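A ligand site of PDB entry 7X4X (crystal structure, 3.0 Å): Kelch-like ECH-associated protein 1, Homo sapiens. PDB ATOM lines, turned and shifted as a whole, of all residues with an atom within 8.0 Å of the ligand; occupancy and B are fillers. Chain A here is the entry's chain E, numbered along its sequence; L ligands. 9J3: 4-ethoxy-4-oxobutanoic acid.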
ATOM      1  N   TYR A  44      -7.538 -24.697 -12.536  1.00  0.00           N
ATOM      2  CA  TYR A  44      -8.481 -25.461 -11.729  1.00  0.00           C
ATOM      3  C   TYR A  44      -9.189 -26.479 -12.612  1.00  0.00           C
ATOM      4  O   TYR A  44      -9.469 -26.208 -13.785  1.00  0.00           O
ATOM      5  CB  TYR A  44      -9.504 -24.547 -11.057  1.00  0.00           C
ATOM      6  CG  TYR A  44      -9.954 -25.013  -9.686  1.00  0.00           C
ATOM      7  CD1 TYR A  44      -9.047 -25.554  -8.786  1.00  0.00           C
ATOM      8  CD2 TYR A  44     -11.284 -24.899  -9.293  1.00  0.00           C
ATOM      9  CE1 TYR A  44      -9.452 -25.987  -7.530  1.00  0.00           C
ATOM     10  CE2 TYR A  44     -11.697 -25.325  -8.046  1.00  0.00           C
ATOM     11  CZ  TYR A  44     -10.772 -25.863  -7.162  1.00  0.00           C
ATOM     12  OH  TYR A  44     -11.186 -26.289  -5.915  1.00  0.00           O
ATOM     13  N   GLN A  45      -9.469 -27.654 -12.050  1.00  0.00           N
ATOM     14  CA  GLN A  45     -10.128 -28.711 -12.801  1.00  0.00           C
ATOM     15  C   GLN A  45     -11.489 -28.254 -13.298  1.00  0.00           C
ATOM     16  O   GLN A  45     -12.299 -27.728 -12.520  1.00  0.00           O
ATOM     17  CB  GLN A  45     -10.276 -29.966 -11.932  1.00  0.00           C
ATOM     18  N   ASP A  46     -11.733 -28.438 -14.588  1.00  0.00           N
ATOM     19  CA  ASP A  46     -12.961 -28.007 -15.248  1.00  0.00           C
ATOM     20  C   ASP A  46     -13.180 -26.502 -15.077  1.00  0.00           C
ATOM     21  O   ASP A  46     -14.176 -26.045 -14.525  1.00  0.00           O
ATOM     22  CB  ASP A  46     -14.165 -28.803 -14.738  1.00  0.00           C
ATOM     23  CG  ASP A  46     -14.115 -30.261 -15.147  1.00  0.00           C
ATOM     24  OD1 ASP A  46     -13.714 -30.543 -16.301  1.00  0.00           O
ATOM     25  OD2 ASP A  46     -14.480 -31.123 -14.327  1.00  0.00           O
ATOM     26  N   ALA A  47     -12.195 -25.729 -15.558  1.00  0.00           N
ATOM     27  CA  ALA A  47     -12.241 -24.282 -15.475  1.00  0.00           C
ATOM     28  C   ALA A  47     -11.295 -23.705 -16.511  1.00  0.00           C
ATOM     29  O   ALA A  47     -10.212 -24.266 -16.717  1.00  0.00           O
ATOM     30  CB  ALA A  47     -11.857 -23.786 -14.078  1.00  0.00           C
ATOM     31  N   ILE A  87      -6.938 -23.672  -6.251  1.00  0.00           N
ATOM     32  CA  ILE A  87      -7.798 -22.518  -6.067  1.00  0.00           C
ATOM     33  C   ILE A  87      -8.379 -22.112  -7.418  1.00  0.00           C
ATOM     34  O   ILE A  87      -7.679 -22.163  -8.439  1.00  0.00           O
ATOM     35  CB  ILE A  87      -7.059 -21.345  -5.392  1.00  0.00           C
ATOM     36  CG1 ILE A  87      -7.999 -20.168  -5.138  1.00  0.00           C
ATOM     37  CG2 ILE A  87      -5.858 -20.919  -6.217  1.00  0.00           C
ATOM     38  CD1 ILE A  87      -7.369 -19.030  -4.381  1.00  0.00           C
ATOM     39  N   HIS A  88      -9.652 -21.748  -7.427  1.00  0.00           N
ATOM     40  CA  HIS A  88     -10.323 -21.391  -8.654  1.00  0.00           C
ATOM     41  C   HIS A  88      -9.849 -20.026  -9.155  1.00  0.00           C
ATOM     42  O   HIS A  88      -9.548 -19.135  -8.355  1.00  0.00           O
ATOM     43  CB  HIS A  88     -11.839 -21.381  -8.447  1.00  0.00           C
ATOM     44  CG  HIS A  88     -12.623 -21.199  -9.699  1.00  0.00           C
ATOM     45  ND1 HIS A  88     -13.142 -19.972 -10.084  1.00  0.00           N
ATOM     46  CD2 HIS A  88     -12.987 -22.078 -10.663  1.00  0.00           C
ATOM     47  CE1 HIS A  88     -13.792 -20.110 -11.231  1.00  0.00           C
ATOM     48  NE2 HIS A  88     -13.714 -21.375 -11.608  1.00  0.00           N
ATOM     49  N   PRO A  89      -9.760 -19.835 -10.475  1.00  0.00           N
ATOM     50  CA  PRO A  89      -9.328 -18.528 -11.007  1.00  0.00           C
ATOM     51  C   PRO A  89     -10.156 -17.357 -10.504  1.00  0.00           C
ATOM     52  O   PRO A  89      -9.587 -16.299 -10.198  1.00  0.00           O
ATOM     53  CB  PRO A  89      -9.471 -18.713 -12.525  1.00  0.00           C
ATOM     54  CG  PRO A  89      -9.304 -20.173 -12.747  1.00  0.00           C
ATOM     55  CD  PRO A  89      -9.900 -20.854 -11.534  1.00  0.00           C
ATOM     56  N   LYS A  90     -11.476 -17.512 -10.420  1.00  0.00           N
ATOM     57  CA  LYS A  90     -12.306 -16.424  -9.928  1.00  0.00           C
ATOM     58  C   LYS A  90     -11.962 -16.060  -8.487  1.00  0.00           C
ATOM     59  O   LYS A  90     -12.025 -14.892  -8.104  1.00  0.00           O
ATOM     60  CB  LYS A  90     -13.789 -16.787 -10.039  1.00  0.00           C
ATOM     61  N   VAL A  91     -11.565 -17.050  -7.678  1.00  0.00           N
ATOM     62  CA  VAL A  91     -11.192 -16.769  -6.292  1.00  0.00           C
ATOM     63  C   VAL A  91      -9.821 -16.112  -6.224  1.00  0.00           C
ATOM     64  O   VAL A  91      -9.626 -15.150  -5.466  1.00  0.00           O
ATOM     65  CB  VAL A  91     -11.248 -18.068  -5.463  1.00  0.00           C
ATOM     66  CG1 VAL A  91     -10.777 -17.797  -4.045  1.00  0.00           C
ATOM     67  CG2 VAL A  91     -12.652 -18.638  -5.468  1.00  0.00           C
ATOM     68  N   MET A  92      -8.862 -16.599  -7.004  1.00  0.00           N
ATOM     69  CA  MET A  92      -7.549 -15.951  -7.074  1.00  0.00           C
ATOM     70  C   MET A  92      -7.664 -14.506  -7.559  1.00  0.00           C
ATOM     71  O   MET A  92      -6.810 -13.674  -7.224  1.00  0.00           O
ATOM     72  CB  MET A  92      -6.608 -16.752  -7.981  1.00  0.00           C
ATOM     73  CG  MET A  92      -5.230 -16.126  -8.166  1.00  0.00           C
ATOM     74  SD  MET A  92      -4.260 -15.939  -6.661  1.00  0.00           S
ATOM     75  CE  MET A  92      -4.420 -17.572  -5.934  1.00  0.00           C
ATOM     76  N   GLU A  93      -8.702 -14.194  -8.319  1.00  0.00           N
ATOM     77  CA  GLU A  93      -8.904 -12.822  -8.778  1.00  0.00           C
ATOM     78  C   GLU A  93      -9.349 -11.921  -7.629  1.00  0.00           C
ATOM     79  O   GLU A  93      -8.828 -10.814  -7.458  1.00  0.00           O
ATOM     80  CB  GLU A  93      -9.925 -12.787  -9.911  1.00  0.00           C
ATOM     81  CG  GLU A  93     -10.470 -11.404 -10.227  1.00  0.00           C
ATOM     82  CD  GLU A  93     -11.568 -11.431 -11.261  1.00  0.00           C
ATOM     83  OE1 GLU A  93     -11.350 -12.011 -12.355  1.00  0.00           O
ATOM     84  OE2 GLU A  93     -12.652 -10.886 -10.997  1.00  0.00           O
ATOM     85  N   ARG A  94     -10.305 -12.373  -6.820  1.00  0.00           N
ATOM     86  CA  ARG A  94     -10.776 -11.554  -5.706  1.00  0.00           C
ATOM     87  C   ARG A  94      -9.689 -11.339  -4.672  1.00  0.00           C
ATOM     88  O   ARG A  94      -9.639 -10.290  -4.022  1.00  0.00           O
ATOM     89  CB  ARG A  94     -12.006 -12.184  -5.032  1.00  0.00           C
ATOM     90  CG  ARG A  94     -12.939 -12.951  -5.960  1.00  0.00           C
ATOM     91  CD  ARG A  94     -13.479 -12.098  -7.089  1.00  0.00           C
ATOM     92  NE  ARG A  94     -14.710 -11.405  -6.730  1.00  0.00           N
ATOM     93  CZ  ARG A  94     -15.856 -11.531  -7.394  1.00  0.00           C
ATOM     94  NH1 ARG A  94     -15.962 -12.335  -8.442  1.00  0.00           N
ATOM     95  NH2 ARG A  94     -16.917 -10.835  -6.995  1.00  0.00           N
ATOM     96  N   ILE A 104     -13.079  -6.374  -1.111  1.00  0.00           N
ATOM     97  CA  ILE A 104     -13.400  -7.672  -1.674  1.00  0.00           C
ATOM     98  C   ILE A 104     -14.913  -7.821  -1.708  1.00  0.00           C
ATOM     99  O   ILE A 104     -15.597  -7.559  -0.708  1.00  0.00           O
ATOM    100  CB  ILE A 104     -12.744  -8.812  -0.862  1.00  0.00           C
ATOM    101  CG1 ILE A 104     -13.296 -10.170  -1.284  1.00  0.00           C
ATOM    102  CG2 ILE A 104     -12.941  -8.596   0.632  1.00  0.00           C
ATOM    103  CD1 ILE A 104     -12.318 -11.304  -1.094  1.00  0.00           C
ATOM    104  N   SER A 105     -15.446  -8.229  -2.858  1.00  0.00           N
ATOM    105  CA  SER A 105     -16.889  -8.311  -3.073  1.00  0.00           C
ATOM    106  C   SER A 105     -17.204  -9.511  -3.940  1.00  0.00           C
ATOM    107  O   SER A 105     -16.743  -9.583  -5.091  1.00  0.00           O
ATOM    108  CB  SER A 105     -17.416  -7.027  -3.713  1.00  0.00           C
ATOM    109  OG  SER A 105     -18.822  -7.056  -3.860  1.00  0.00           O
ATOM    110  N   MET A 106     -18.001 -10.445  -3.416  1.00  0.00           N
ATOM    111  CA  MET A 106     -18.404 -11.639  -4.160  1.00  0.00           C
ATOM    112  C   MET A 106     -19.879 -11.907  -3.881  1.00  0.00           C
ATOM    113  O   MET A 106     -20.554 -11.155  -3.178  1.00  0.00           O
ATOM    114  CB  MET A 106     -17.523 -12.844  -3.776  1.00  0.00           C
ATOM    115  CG  MET A 106     -18.005 -13.642  -2.569  1.00  0.00           C
ATOM    116  SD  MET A 106     -17.508 -12.958  -0.980  1.00  0.00           S
ATOM    117  CE  MET A 106     -15.797 -12.578  -1.311  1.00  0.00           C
ATOM    118  N   GLY A 107     -20.392 -13.003  -4.473  1.00  0.00           N
ATOM    119  CA  GLY A 107     -21.773 -13.409  -4.248  1.00  0.00           C
ATOM    120  C   GLY A 107     -21.933 -14.328  -3.043  1.00  0.00           C
ATOM    121  O   GLY A 107     -20.966 -14.787  -2.435  1.00  0.00           O
ATOM    122  N   GLU A 108     -23.197 -14.599  -2.712  1.00  0.00           N
ATOM    123  CA  GLU A 108     -23.501 -15.402  -1.530  1.00  0.00           C
ATOM    124  C   GLU A 108     -23.012 -16.832  -1.667  1.00  0.00           C
ATOM    125  O   GLU A 108     -22.676 -17.474  -0.665  1.00  0.00           O
ATOM    126  CB  GLU A 108     -25.004 -15.384  -1.257  1.00  0.00           C
ATOM    127  CG  GLU A 108     -25.400 -15.699   0.180  1.00  0.00           C
ATOM    128  CD  GLU A 108     -26.876 -15.987   0.320  1.00  0.00           C
ATOM    129  OE1 GLU A 108     -27.577 -16.022  -0.706  1.00  0.00           O
ATOM    130  OE2 GLU A 108     -27.345 -16.171   1.469  1.00  0.00           O
ATOM    131  N   LYS A 109     -22.949 -17.347  -2.889  1.00  0.00           N
ATOM    132  CA  LYS A 109     -22.584 -18.737  -3.136  1.00  0.00           C
ATOM    133  C   LYS A 109     -21.082 -18.940  -3.307  1.00  0.00           C
ATOM    134  O   LYS A 109     -20.659 -20.029  -3.733  1.00  0.00           O
ATOM    135  CB  LYS A 109     -23.313 -19.258  -4.373  1.00  0.00           C
ATOM    136  N   CYS A 110     -20.269 -17.942  -2.975  1.00  0.00           N
ATOM    137  CA  CYS A 110     -18.827 -18.046  -3.152  1.00  0.00           C
ATOM    138  C   CYS A 110     -18.020 -17.603  -1.934  1.00  0.00           C
ATOM    139  O   CYS A 110     -16.790 -17.623  -1.994  1.00  0.00           O
ATOM    140  CB  CYS A 110     -18.366 -17.221  -4.372  1.00  0.00           C
ATOM    141  SG  CYS A 110     -19.702 -16.372  -5.233  1.00  0.00           S
ATOM    142  N   VAL A 111     -18.678 -17.221  -0.843  1.00  0.00           N
ATOM    143  CA  VAL A 111     -17.960 -16.767   0.346  1.00  0.00           C
ATOM    144  C   VAL A 111     -17.094 -17.898   0.908  1.00  0.00           C
ATOM    145  O   VAL A 111     -15.950 -17.673   1.313  1.00  0.00           O
ATOM    146  CB  VAL A 111     -18.940 -16.237   1.402  1.00  0.00           C
ATOM    147  CG1 VAL A 111     -18.211 -15.403   2.436  1.00  0.00           C
ATOM    148  CG2 VAL A 111     -20.031 -15.428   0.730  1.00  0.00           C
ATOM    149  N   LEU A 112     -17.627 -19.121   0.912  1.00  0.00           N
ATOM    150  CA  LEU A 112     -16.855 -20.257   1.413  1.00  0.00           C
ATOM    151  C   LEU A 112     -15.629 -20.517   0.542  1.00  0.00           C
ATOM    152  O   LEU A 112     -14.545 -20.799   1.065  1.00  0.00           O
ATOM    153  CB  LEU A 112     -17.742 -21.499   1.471  1.00  0.00           C
ATOM    154  CG  LEU A 112     -17.211 -22.777   2.123  1.00  0.00           C
ATOM    155  CD1 LEU A 112     -16.247 -22.472   3.270  1.00  0.00           C
ATOM    156  CD2 LEU A 112     -18.355 -23.655   2.606  1.00  0.00           C
ATOM    157  N   HIS A 113     -15.780 -20.409  -0.779  1.00  0.00           N
ATOM    158  CA  HIS A 113     -14.652 -20.632  -1.671  1.00  0.00           C
ATOM    159  C   HIS A 113     -13.590 -19.555  -1.505  1.00  0.00           C
ATOM    160  O   HIS A 113     -12.387 -19.858  -1.440  1.00  0.00           O
ATOM    161  CB  HIS A 113     -15.135 -20.706  -3.118  1.00  0.00           C
ATOM    162  CG  HIS A 113     -15.893 -21.948  -3.448  1.00  0.00           C
ATOM    163  ND1 HIS A 113     -16.898 -21.988  -4.388  1.00  0.00           N
ATOM    164  CD2 HIS A 113     -15.782 -23.212  -2.955  1.00  0.00           C
ATOM    165  CE1 HIS A 113     -17.373 -23.216  -4.462  1.00  0.00           C
ATOM    166  NE2 HIS A 113     -16.719 -23.969  -3.605  1.00  0.00           N
ATOM    167  N   VAL A 114     -14.018 -18.293  -1.438  1.00  0.00           N
ATOM    168  CA  VAL A 114     -13.067 -17.202  -1.227  1.00  0.00           C
ATOM    169  C   VAL A 114     -12.394 -17.342   0.130  1.00  0.00           C
ATOM    170  O   VAL A 114     -11.180 -17.137   0.262  1.00  0.00           O
ATOM    171  CB  VAL A 114     -13.774 -15.843  -1.370  1.00  0.00           C
ATOM    172  CG1 VAL A 114     -13.079 -14.778  -0.530  1.00  0.00           C
ATOM    173  CG2 VAL A 114     -13.831 -15.426  -2.829  1.00  0.00           C
ATOM    174  N   MET A 115     -13.168 -17.703   1.165  1.00  0.00           N
ATOM    175  CA  MET A 115     -12.587 -17.923   2.487  1.00  0.00           C
ATOM    176  C   MET A 115     -11.537 -19.022   2.452  1.00  0.00           C
ATOM    177  O   MET A 115     -10.485 -18.899   3.080  1.00  0.00           O
ATOM    178  CB  MET A 115     -13.691 -18.261   3.481  1.00  0.00           C
ATOM    179  CG  MET A 115     -13.180 -18.747   4.822  1.00  0.00           C
ATOM    180  SD  MET A 115     -14.517 -19.217   5.942  1.00  0.00           S
ATOM    181  CE  MET A 115     -14.097 -18.255   7.390  1.00  0.00           C
HETATM  182  OAA 9J3 L   1     -16.600 -14.457  -6.372  1.00  0.00           O
HETATM  183  CAC 9J3 L   1     -16.919 -15.370  -7.172  1.00  0.00           C
HETATM  184  OAB 9J3 L   1     -17.882 -15.200  -7.970  1.00  0.00           O
HETATM  185  CAD 9J3 L   1     -16.140 -16.683  -7.186  1.00  0.00           C
HETATM  186  CAE 9J3 L   1     -16.918 -17.831  -7.832  1.00  0.00           C
HETATM  187  CAF 9J3 L   1     -16.634 -19.155  -7.130  1.00  0.00           C
HETATM  188  OAG 9J3 L   1     -16.051 -19.168  -6.094  1.00  0.00           O
HETATM  189  OAH 9J3 L   1     -17.047 -20.365  -7.698  1.00  0.00           O
HETATM  190  CAI 9J3 L   1     -16.073 -20.968  -8.512  1.00  0.00           C
HETATM  191  CAJ 9J3 L   1     -15.792 -22.359  -7.951  1.00  0.00           C
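An oxygen (OAA) of the ligand lies within salt-bridge range of the guanidinium group of Arg 94. A ring nitrogen (ND1) of His 113 sits at hydrogen-bond distance from an oxygen (OAG) of the ligand (3.4 Å). An oxygen (OAB) of the ligand sits at hydrogen-bond distance from the side-chain sulfur of Cys 110, at 3.5 Å.
The backbone carbonyl oxygen of Ser 105 lies close to the guanidinium group of Arg 94, 3.2 Å away. SG of Cys 110 is in hydrogen-bond range of O of Gly 107 (3.5 Å). A ring nitrogen (ND1) of His 88 is in hydrogen-bond range of the backbone NH (N) of Lys 90 (3.0 Å).
His 88 touches the ligand (ND1 to CAI, 3.5 Å). Lys 90 touches the ligand (CB to CAD, 3.7 Å). Val 91 touches the ligand. Met 106 touches the ligand. Of the 24 residues printed, 7 come within 4 Å of the ligand. The nearest printed residue that does not touch the ligand is Gly 107 (4.5 Å).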
